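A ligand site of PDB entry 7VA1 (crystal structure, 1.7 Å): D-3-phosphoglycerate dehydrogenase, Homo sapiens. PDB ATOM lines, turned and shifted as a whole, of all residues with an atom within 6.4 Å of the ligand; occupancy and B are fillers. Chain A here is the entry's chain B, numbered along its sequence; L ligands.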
ATOM      1  N   ILE A  57      -2.120 -23.207  19.704  1.00  0.00           N
ATOM      2  CA  ILE A  57      -3.449 -23.766  19.902  1.00  0.00           C
ATOM      3  C   ILE A  57      -3.714 -23.819  21.408  1.00  0.00           C
ATOM      4  O   ILE A  57      -3.123 -24.653  22.115  1.00  0.00           O
ATOM      5  CB  ILE A  57      -3.571 -25.161  19.296  1.00  0.00           C
ATOM      6  CG1 ILE A  57      -3.154 -25.130  17.818  1.00  0.00           C
ATOM      7  CG2 ILE A  57      -4.994 -25.665  19.471  1.00  0.00           C
ATOM      8  CD1 ILE A  57      -3.214 -26.459  17.152  1.00  0.00           C
ATOM      9  N   LEU A  58      -4.628 -22.975  21.882  1.00  0.00           N
ATOM     10  CA  LEU A  58      -4.963 -22.893  23.308  1.00  0.00           C
ATOM     11  C   LEU A  58      -6.204 -23.724  23.577  1.00  0.00           C
ATOM     12  O   LEU A  58      -7.297 -23.351  23.152  1.00  0.00           O
ATOM     13  CB  LEU A  58      -5.166 -21.439  23.730  1.00  0.00           C
ATOM     14  CG  LEU A  58      -3.939 -20.575  23.413  1.00  0.00           C
ATOM     15  CD1 LEU A  58      -4.053 -19.183  24.001  1.00  0.00           C
ATOM     16  CD2 LEU A  58      -2.645 -21.276  23.852  1.00  0.00           C
ATOM     17  N   GLY A  59      -6.053 -24.845  24.268  1.00  0.00           N
ATOM     18  CA  GLY A  59      -7.158 -25.775  24.419  1.00  0.00           C
ATOM     19  C   GLY A  59      -7.018 -26.931  23.458  1.00  0.00           C
ATOM     20  O   GLY A  59      -7.085 -26.747  22.237  1.00  0.00           O
ATOM     21  N   LEU A  60      -6.751 -28.125  23.984  1.00  0.00           N
ATOM     22  CA  LEU A  60      -6.380 -29.260  23.161  1.00  0.00           C
ATOM     23  C   LEU A  60      -7.373 -30.404  23.307  1.00  0.00           C
ATOM     24  O   LEU A  60      -6.997 -31.571  23.388  1.00  0.00           O
ATOM     25  CB  LEU A  60      -4.963 -29.706  23.485  1.00  0.00           C
ATOM     26  CG  LEU A  60      -3.889 -28.658  23.150  1.00  0.00           C
ATOM     27  CD1 LEU A  60      -2.534 -29.094  23.647  1.00  0.00           C
ATOM     28  CD2 LEU A  60      -3.826 -28.411  21.647  1.00  0.00           C
ATOM     29  N   GLY A  61      -8.664 -30.070  23.345  1.00  0.00           N
ATOM     30  CA  GLY A  61      -9.716 -31.052  23.246  1.00  0.00           C
ATOM     31  C   GLY A  61      -9.917 -31.440  21.791  1.00  0.00           C
ATOM     32  O   GLY A  61      -9.021 -31.278  20.958  1.00  0.00           O
ATOM     33  N   ARG A  62     -11.096 -31.988  21.491  1.00  0.00           N
ATOM     34  CA  ARG A  62     -11.331 -32.572  20.158  1.00  0.00           C
ATOM     35  C   ARG A  62     -11.097 -31.557  19.044  1.00  0.00           C
ATOM     36  O   ARG A  62     -10.459 -31.877  18.027  1.00  0.00           O
ATOM     37  CB  ARG A  62     -12.738 -33.151  20.070  1.00  0.00           C
ATOM     38  CG  ARG A  62     -12.999 -33.876  18.741  1.00  0.00           C
ATOM     39  CD  ARG A  62     -14.386 -34.519  18.685  1.00  0.00           C
ATOM     40  NE  ARG A  62     -14.551 -35.572  19.673  1.00  0.00           N
ATOM     41  CZ  ARG A  62     -15.707 -36.180  19.937  1.00  0.00           C
ATOM     42  NH1 ARG A  62     -16.811 -35.814  19.297  1.00  0.00           N
ATOM     43  NH2 ARG A  62     -15.762 -37.140  20.850  1.00  0.00           N
ATOM     44  N   ARG A  65      -7.478 -30.501  18.550  1.00  0.00           N
ATOM     45  CA  ARG A  65      -6.693 -31.562  17.929  1.00  0.00           C
ATOM     46  C   ARG A  65      -6.972 -31.635  16.430  1.00  0.00           C
ATOM     47  O   ARG A  65      -6.056 -31.857  15.630  1.00  0.00           O
ATOM     48  CB  ARG A  65      -6.994 -32.914  18.565  1.00  0.00           C
ATOM     49  CG  ARG A  65      -6.592 -33.051  20.029  1.00  0.00           C
ATOM     50  CD  ARG A  65      -6.698 -34.509  20.446  1.00  0.00           C
ATOM     51  NE  ARG A  65      -8.071 -34.888  20.777  1.00  0.00           N
ATOM     52  CZ  ARG A  65      -8.589 -34.800  21.998  1.00  0.00           C
ATOM     53  NH1 ARG A  65      -7.841 -34.354  23.005  1.00  0.00           N
ATOM     54  NH2 ARG A  65      -9.838 -35.170  22.216  1.00  0.00           N
ATOM     55  N   GLY A  80       1.129 -25.549  21.795  1.00  0.00           N
ATOM     56  CA  GLY A  80      -0.108 -25.210  22.465  1.00  0.00           C
ATOM     57  C   GLY A  80      -0.037 -25.430  23.957  1.00  0.00           C
ATOM     58  O   GLY A  80       1.005 -25.753  24.520  1.00  0.00           O
ATOM     59  N   TYR A  81      -1.194 -25.223  24.585  1.00  0.00           N
ATOM     60  CA  TYR A  81      -1.292 -25.384  26.021  1.00  0.00           C
ATOM     61  C   TYR A  81      -2.692 -25.891  26.344  1.00  0.00           C
ATOM     62  O   TYR A  81      -3.681 -25.447  25.764  1.00  0.00           O
ATOM     63  CB  TYR A  81      -1.013 -24.075  26.756  1.00  0.00           C
ATOM     64  CG  TYR A  81      -1.062 -24.234  28.251  1.00  0.00           C
ATOM     65  CD1 TYR A  81      -0.019 -24.851  28.923  1.00  0.00           C
ATOM     66  CD2 TYR A  81      -2.145 -23.796  28.984  1.00  0.00           C
ATOM     67  CE1 TYR A  81      -0.055 -25.021  30.288  1.00  0.00           C
ATOM     68  CE2 TYR A  81      -2.190 -23.959  30.357  1.00  0.00           C
ATOM     69  CZ  TYR A  81      -1.136 -24.571  31.000  1.00  0.00           C
ATOM     70  OH  TYR A  81      -1.172 -24.741  32.366  1.00  0.00           O
ATOM     71  N   ASP A  82      -2.748 -26.801  27.300  1.00  0.00           N
ATOM     72  CA  ASP A  82      -3.996 -27.291  27.861  1.00  0.00           C
ATOM     73  C   ASP A  82      -3.656 -27.828  29.234  1.00  0.00           C
ATOM     74  O   ASP A  82      -2.854 -28.758  29.345  1.00  0.00           O
ATOM     75  CB  ASP A  82      -4.606 -28.400  27.014  1.00  0.00           C
ATOM     76  CG  ASP A  82      -5.996 -28.790  27.477  1.00  0.00           C
ATOM     77  OD1 ASP A  82      -6.104 -29.390  28.569  1.00  0.00           O
ATOM     78  OD2 ASP A  82      -6.973 -28.503  26.756  1.00  0.00           O
ATOM     79  N   PRO A  83      -4.250 -27.305  30.304  1.00  0.00           N
ATOM     80  CA  PRO A  83      -3.855 -27.760  31.645  1.00  0.00           C
ATOM     81  C   PRO A  83      -4.379 -29.139  32.002  1.00  0.00           C
ATOM     82  O   PRO A  83      -3.972 -29.691  33.031  1.00  0.00           O
ATOM     83  CB  PRO A  83      -4.439 -26.680  32.563  1.00  0.00           C
ATOM     84  CG  PRO A  83      -5.668 -26.225  31.819  1.00  0.00           C
ATOM     85  CD  PRO A  83      -5.259 -26.238  30.355  1.00  0.00           C
ATOM     86  N   ILE A  84      -5.228 -29.733  31.171  1.00  0.00           N
ATOM     87  CA  ILE A  84      -5.735 -31.077  31.414  1.00  0.00           C
ATOM     88  C   ILE A  84      -4.856 -32.144  30.748  1.00  0.00           C
ATOM     89  O   ILE A  84      -4.729 -33.251  31.281  1.00  0.00           O
ATOM     90  CB  ILE A  84      -7.182 -31.190  30.922  1.00  0.00           C
ATOM     91  CG1 ILE A  84      -7.998 -30.021  31.473  1.00  0.00           C
ATOM     92  CG2 ILE A  84      -7.793 -32.545  31.241  1.00  0.00           C
ATOM     93  CD1 ILE A  84      -8.018 -29.992  32.988  1.00  0.00           C
ATOM     94  N   ILE A  85      -4.266 -31.816  29.619  1.00  0.00           N
ATOM     95  CA  ILE A  85      -3.503 -32.764  28.816  1.00  0.00           C
ATOM     96  C   ILE A  85      -2.035 -32.667  29.181  1.00  0.00           C
ATOM     97  O   ILE A  85      -1.490 -31.556  29.312  1.00  0.00           O
ATOM     98  CB  ILE A  85      -3.727 -32.459  27.318  1.00  0.00           C
ATOM     99  CG1 ILE A  85      -5.223 -32.473  26.999  1.00  0.00           C
ATOM    100  CG2 ILE A  85      -2.938 -33.402  26.427  1.00  0.00           C
ATOM    101  CD1 ILE A  85      -5.854 -33.839  27.173  1.00  0.00           C
ATOM    102  N   VAL A  89       0.914 -36.620  26.004  1.00  0.00           N
ATOM    103  CA  VAL A  89      -0.311 -36.858  25.228  1.00  0.00           C
ATOM    104  C   VAL A  89      -0.381 -35.910  24.041  1.00  0.00           C
ATOM    105  O   VAL A  89      -0.692 -36.314  22.917  1.00  0.00           O
ATOM    106  CB  VAL A  89      -1.554 -36.709  26.126  1.00  0.00           C
ATOM    107  CG1 VAL A  89      -2.828 -36.826  25.295  1.00  0.00           C
ATOM    108  CG2 VAL A  89      -1.550 -37.734  27.261  1.00  0.00           C
ATOM    109  N   PHE A  93      -0.344 -36.268  19.229  1.00  0.00           N
ATOM    110  CA  PHE A  93      -0.970 -35.672  18.056  1.00  0.00           C
ATOM    111  C   PHE A  93      -0.212 -34.436  17.562  1.00  0.00           C
ATOM    112  O   PHE A  93      -0.802 -33.565  16.911  1.00  0.00           O
ATOM    113  CB  PHE A  93      -2.462 -35.376  18.280  1.00  0.00           C
ATOM    114  CG  PHE A  93      -2.785 -34.603  19.526  1.00  0.00           C
ATOM    115  CD1 PHE A  93      -2.794 -33.206  19.527  1.00  0.00           C
ATOM    116  CD2 PHE A  93      -3.160 -35.270  20.684  1.00  0.00           C
ATOM    117  CE1 PHE A  93      -3.120 -32.506  20.680  1.00  0.00           C
ATOM    118  CE2 PHE A  93      -3.478 -34.575  21.839  1.00  0.00           C
ATOM    119  CZ  PHE A  93      -3.463 -33.183  21.835  1.00  0.00           C
ATOM    120  N   LEU A 100       2.126 -21.295  28.984  1.00  0.00           N
ATOM    121  CA  LEU A 100       1.504 -20.192  28.267  1.00  0.00           C
ATOM    122  C   LEU A 100       2.495 -19.060  27.999  1.00  0.00           C
ATOM    123  O   LEU A 100       2.515 -18.495  26.907  1.00  0.00           O
ATOM    124  CB  LEU A 100       0.300 -19.630  29.036  1.00  0.00           C
ATOM    125  CG  LEU A 100      -1.068 -20.215  28.730  1.00  0.00           C
ATOM    126  CD1 LEU A 100      -2.141 -19.451  29.454  1.00  0.00           C
ATOM    127  CD2 LEU A 100      -1.311 -20.167  27.232  1.00  0.00           C
ATOM    128  N   HIS A 113      -9.514 -22.800  21.597  1.00  0.00           N
ATOM    129  CA  HIS A 113     -10.433 -23.926  21.559  1.00  0.00           C
ATOM    130  C   HIS A 113     -10.674 -24.439  22.965  1.00  0.00           C
ATOM    131  O   HIS A 113     -10.770 -25.647  23.208  1.00  0.00           O
ATOM    132  CB  HIS A 113      -9.897 -25.020  20.645  1.00  0.00           C
ATOM    133  CG  HIS A 113      -9.689 -24.531  19.247  1.00  0.00           C
ATOM    134  ND1 HIS A 113     -10.750 -24.222  18.427  1.00  0.00           N
ATOM    135  CD2 HIS A 113      -8.567 -24.210  18.565  1.00  0.00           C
ATOM    136  CE1 HIS A 113     -10.301 -23.744  17.285  1.00  0.00           C
ATOM    137  NE2 HIS A 113      -8.975 -23.734  17.331  1.00  0.00           N
ATOM    138  N   THR A 114     -10.800 -23.540  23.891  1.00  0.00           N
ATOM    139  CA  THR A 114     -11.126 -23.846  25.276  1.00  0.00           C
ATOM    140  C   THR A 114     -12.622 -23.695  25.508  1.00  0.00           C
ATOM    141  O   THR A 114     -13.321 -22.993  24.759  1.00  0.00           O
ATOM    142  CB  THR A 114     -10.394 -22.885  26.214  1.00  0.00           C
ATOM    143  OG1 THR A 114     -10.927 -21.570  26.026  1.00  0.00           O
ATOM    144  CG2 THR A 114      -8.938 -22.861  25.942  1.00  0.00           C
ATOM    145  N   PRO A 115     -13.154 -24.324  26.553  1.00  0.00           N
ATOM    146  CA  PRO A 115     -14.480 -23.924  27.006  1.00  0.00           C
ATOM    147  C   PRO A 115     -14.413 -22.491  27.496  1.00  0.00           C
ATOM    148  O   PRO A 115     -13.325 -21.951  27.740  1.00  0.00           O
ATOM    149  CB  PRO A 115     -14.789 -24.883  28.173  1.00  0.00           C
ATOM    150  CG  PRO A 115     -13.738 -25.944  28.127  1.00  0.00           C
ATOM    151  CD  PRO A 115     -12.543 -25.356  27.412  1.00  0.00           C
ATOM    152  N   LEU A 117     -14.787 -20.457  30.522  1.00  0.00           N
ATOM    153  CA  LEU A 117     -14.687 -20.674  31.957  1.00  0.00           C
ATOM    154  C   LEU A 117     -14.155 -19.412  32.608  1.00  0.00           C
ATOM    155  O   LEU A 117     -13.712 -18.495  31.919  1.00  0.00           O
ATOM    156  CB  LEU A 117     -13.758 -21.865  32.266  1.00  0.00           C
ATOM    157  CG  LEU A 117     -14.075 -23.244  31.677  1.00  0.00           C
ATOM    158  CD1 LEU A 117     -12.846 -24.172  31.746  1.00  0.00           C
ATOM    159  CD2 LEU A 117     -15.245 -23.861  32.410  1.00  0.00           C
ATOM    160  N   SER A 119     -11.338 -19.201  34.093  1.00  0.00           N
ATOM    161  CA  SER A 119      -9.927 -19.170  33.721  1.00  0.00           C
ATOM    162  C   SER A 119      -9.694 -18.773  32.267  1.00  0.00           C
ATOM    163  O   SER A 119      -8.570 -18.413  31.927  1.00  0.00           O
ATOM    164  CB  SER A 119      -9.273 -20.509  34.003  1.00  0.00           C
ATOM    165  OG  SER A 119      -9.880 -21.545  33.249  1.00  0.00           O
ATOM    166  N   THR A 120     -10.703 -18.884  31.398  1.00  0.00           N
ATOM    167  CA  THR A 120     -10.502 -18.612  29.965  1.00  0.00           C
ATOM    168  C   THR A 120     -11.182 -17.355  29.464  1.00  0.00           C
ATOM    169  O   THR A 120     -11.018 -17.005  28.291  1.00  0.00           O
ATOM    170  CB  THR A 120     -10.973 -19.808  29.122  1.00  0.00           C
ATOM    171  OG1 THR A 120     -12.386 -19.976  29.266  1.00  0.00           O
ATOM    172  CG2 THR A 120     -10.239 -21.092  29.533  1.00  0.00           C
ATOM    173  N   LEU A 123      -8.631 -14.743  28.120  1.00  0.00           N
ATOM    174  CA  LEU A 123      -7.364 -15.455  28.005  1.00  0.00           C
ATOM    175  C   LEU A 123      -6.350 -14.639  27.209  1.00  0.00           C
ATOM    176  O   LEU A 123      -5.189 -14.507  27.600  1.00  0.00           O
ATOM    177  CB  LEU A 123      -7.627 -16.810  27.370  1.00  0.00           C
ATOM    178  CG  LEU A 123      -6.479 -17.805  27.322  1.00  0.00           C
ATOM    179  CD1 LEU A 123      -5.935 -18.119  28.721  1.00  0.00           C
ATOM    180  CD2 LEU A 123      -6.951 -19.061  26.609  1.00  0.00           C
HETATM  181  C1  LIG L   1      -7.224 -23.685  29.268  1.00  0.00           C
HETATM  182  N1  LIG L   1     -10.312 -35.478  27.409  1.00  0.00           N
HETATM  183  C2  LIG L   1      -6.130 -21.740  30.210  1.00  0.00           C
HETATM  184  C3  LIG L   1      -5.387 -21.633  29.043  1.00  0.00           C
HETATM  185  C4  LIG L   1      -9.211 -24.748  30.373  1.00  0.00           C
HETATM  186  C5  LIG L   1      -6.458 -23.593  28.116  1.00  0.00           C
HETATM  187  C6  LIG L   1     -10.224 -28.936  28.661  1.00  0.00           C
HETATM  188  C7  LIG L   1     -10.203 -30.249  27.966  1.00  0.00           C
HETATM  189  C8  LIG L   1     -11.333 -31.037  28.125  1.00  0.00           C
HETATM  190  C9  LIG L   1     -11.421 -32.284  27.547  1.00  0.00           C
HETATM  191  C10 LIG L   1     -10.364 -32.766  26.794  1.00  0.00           C
HETATM  192  C11 LIG L   1      -9.217 -31.990  26.639  1.00  0.00           C
HETATM  193  C12 LIG L   1      -9.126 -30.733  27.227  1.00  0.00           C
HETATM  194  C13 LIG L   1      -9.043 -36.164  27.648  1.00  0.00           C
HETATM  195  C14 LIG L   1      -8.457 -36.152  28.910  1.00  0.00           C
HETATM  196  C15 LIG L   1      -7.248 -36.807  29.125  1.00  0.00           C
HETATM  197  C16 LIG L   1      -6.618 -37.466  28.078  1.00  0.00           C
HETATM  198  C17 LIG L   1      -7.188 -37.476  26.809  1.00  0.00           C
HETATM  199  C18 LIG L   1      -8.405 -36.828  26.604  1.00  0.00           C
HETATM  200  C19 LIG L   1      -6.534 -38.190  25.662  1.00  0.00           C
HETATM  201  C20 LIG L   1      -6.782 -37.608  24.298  1.00  0.00           C
HETATM  202  C21 LIG L   1      -7.059 -22.772  30.322  1.00  0.00           C
HETATM  203  C22 LIG L   1      -5.546 -22.550  28.000  1.00  0.00           C
HETATM  204  C23 LIG L   1      -8.203 -24.790  29.422  1.00  0.00           C
HETATM  205  C24 LIG L   1      -9.076 -26.741  28.967  1.00  0.00           C
HETATM  206  F1  LIG L   1      -4.813 -22.460  26.874  1.00  0.00           F
HETATM  207  N2  LIG L   1      -8.127 -25.886  28.677  1.00  0.00           N
HETATM  208  N3  LIG L   1      -9.252 -28.060  28.342  1.00  0.00           N
HETATM  209  O1  LIG L   1     -11.095 -28.709  29.499  1.00  0.00           O
HETATM  210  O2  LIG L   1     -11.912 -34.498  25.626  1.00  0.00           O
HETATM  211  O3  LIG L   1      -9.395 -34.559  25.143  1.00  0.00           O
HETATM  212  O4  LIG L   1      -5.830 -39.185  25.826  1.00  0.00           O
HETATM  213  S1  LIG L   1     -10.114 -26.218  30.249  1.00  0.00           S
HETATM  214  S2  LIG L   1     -10.524 -34.381  26.067  1.00  0.00           S
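The guanidinium group of Arg 65 lies within hydrogen-bond range of the backbone carbonyl oxygen of Leu 60 (2.9 Å).
OD1 of Asp 82 lies within hydrogen-bond range of N of Ile 84 (2.8 Å).
N of Ile 85 is in hydrogen-bond range of OD1 of Asp 82 (3.2 Å).
The side-chain carboxylate of Asp 82 lies within hydrogen-bond range of the backbone NH of Leu 60, 2.8 Å away.
O of Leu 58 is in hydrogen-bond range of N of His 113 (2.8 Å).
The backbone NH of Gly 59 lies within hydrogen-bond range of the backbone carbonyl oxygen of Tyr 81 (2.9 Å).
The backbone NH (N) of Tyr 81 sits at hydrogen-bond distance from the backbone carbonyl oxygen (O) of Ile 57, 3.2 Å away.
The side-chain hydroxyl (OG1) of Thr 120 is in hydrogen-bond range of the backbone carbonyl oxygen (O) of Pro 115 (2.7 Å).
The backbone carbonyl oxygen (O) of Tyr 81 lies close to a fluorine (F1) of the ligand (3.4 Å).
Residues that only touch the ligand: Leu 58 (3.3 Å), Pro 83 (3.3 Å), Thr 114 (3.4 Å), Gly 61 (3.6 Å), Leu 123 (3.6 Å), Thr 120 (3.7 Å), Leu 117 (3.7 Å), Gly 59 (3.7 Å), Ile 84 (3.7 Å), Ile 85 (3.8 Å), Pro 115 (3.8 Å), Val 89 (3.9 Å), Leu 100 (3.9 Å) and Leu 60 (3.96 Å).
Of the 23 residues printed, 17 come within 4 Å of the ligand.
The guanidinium group of Arg 65 sits at hydrogen-bond distance from an oxygen (O3) of the ligand (2.7 Å).
A nitrogen (N3) of the ligand is in hydrogen-bond range of the side-chain carboxylate of Asp 82 (2.8 Å).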
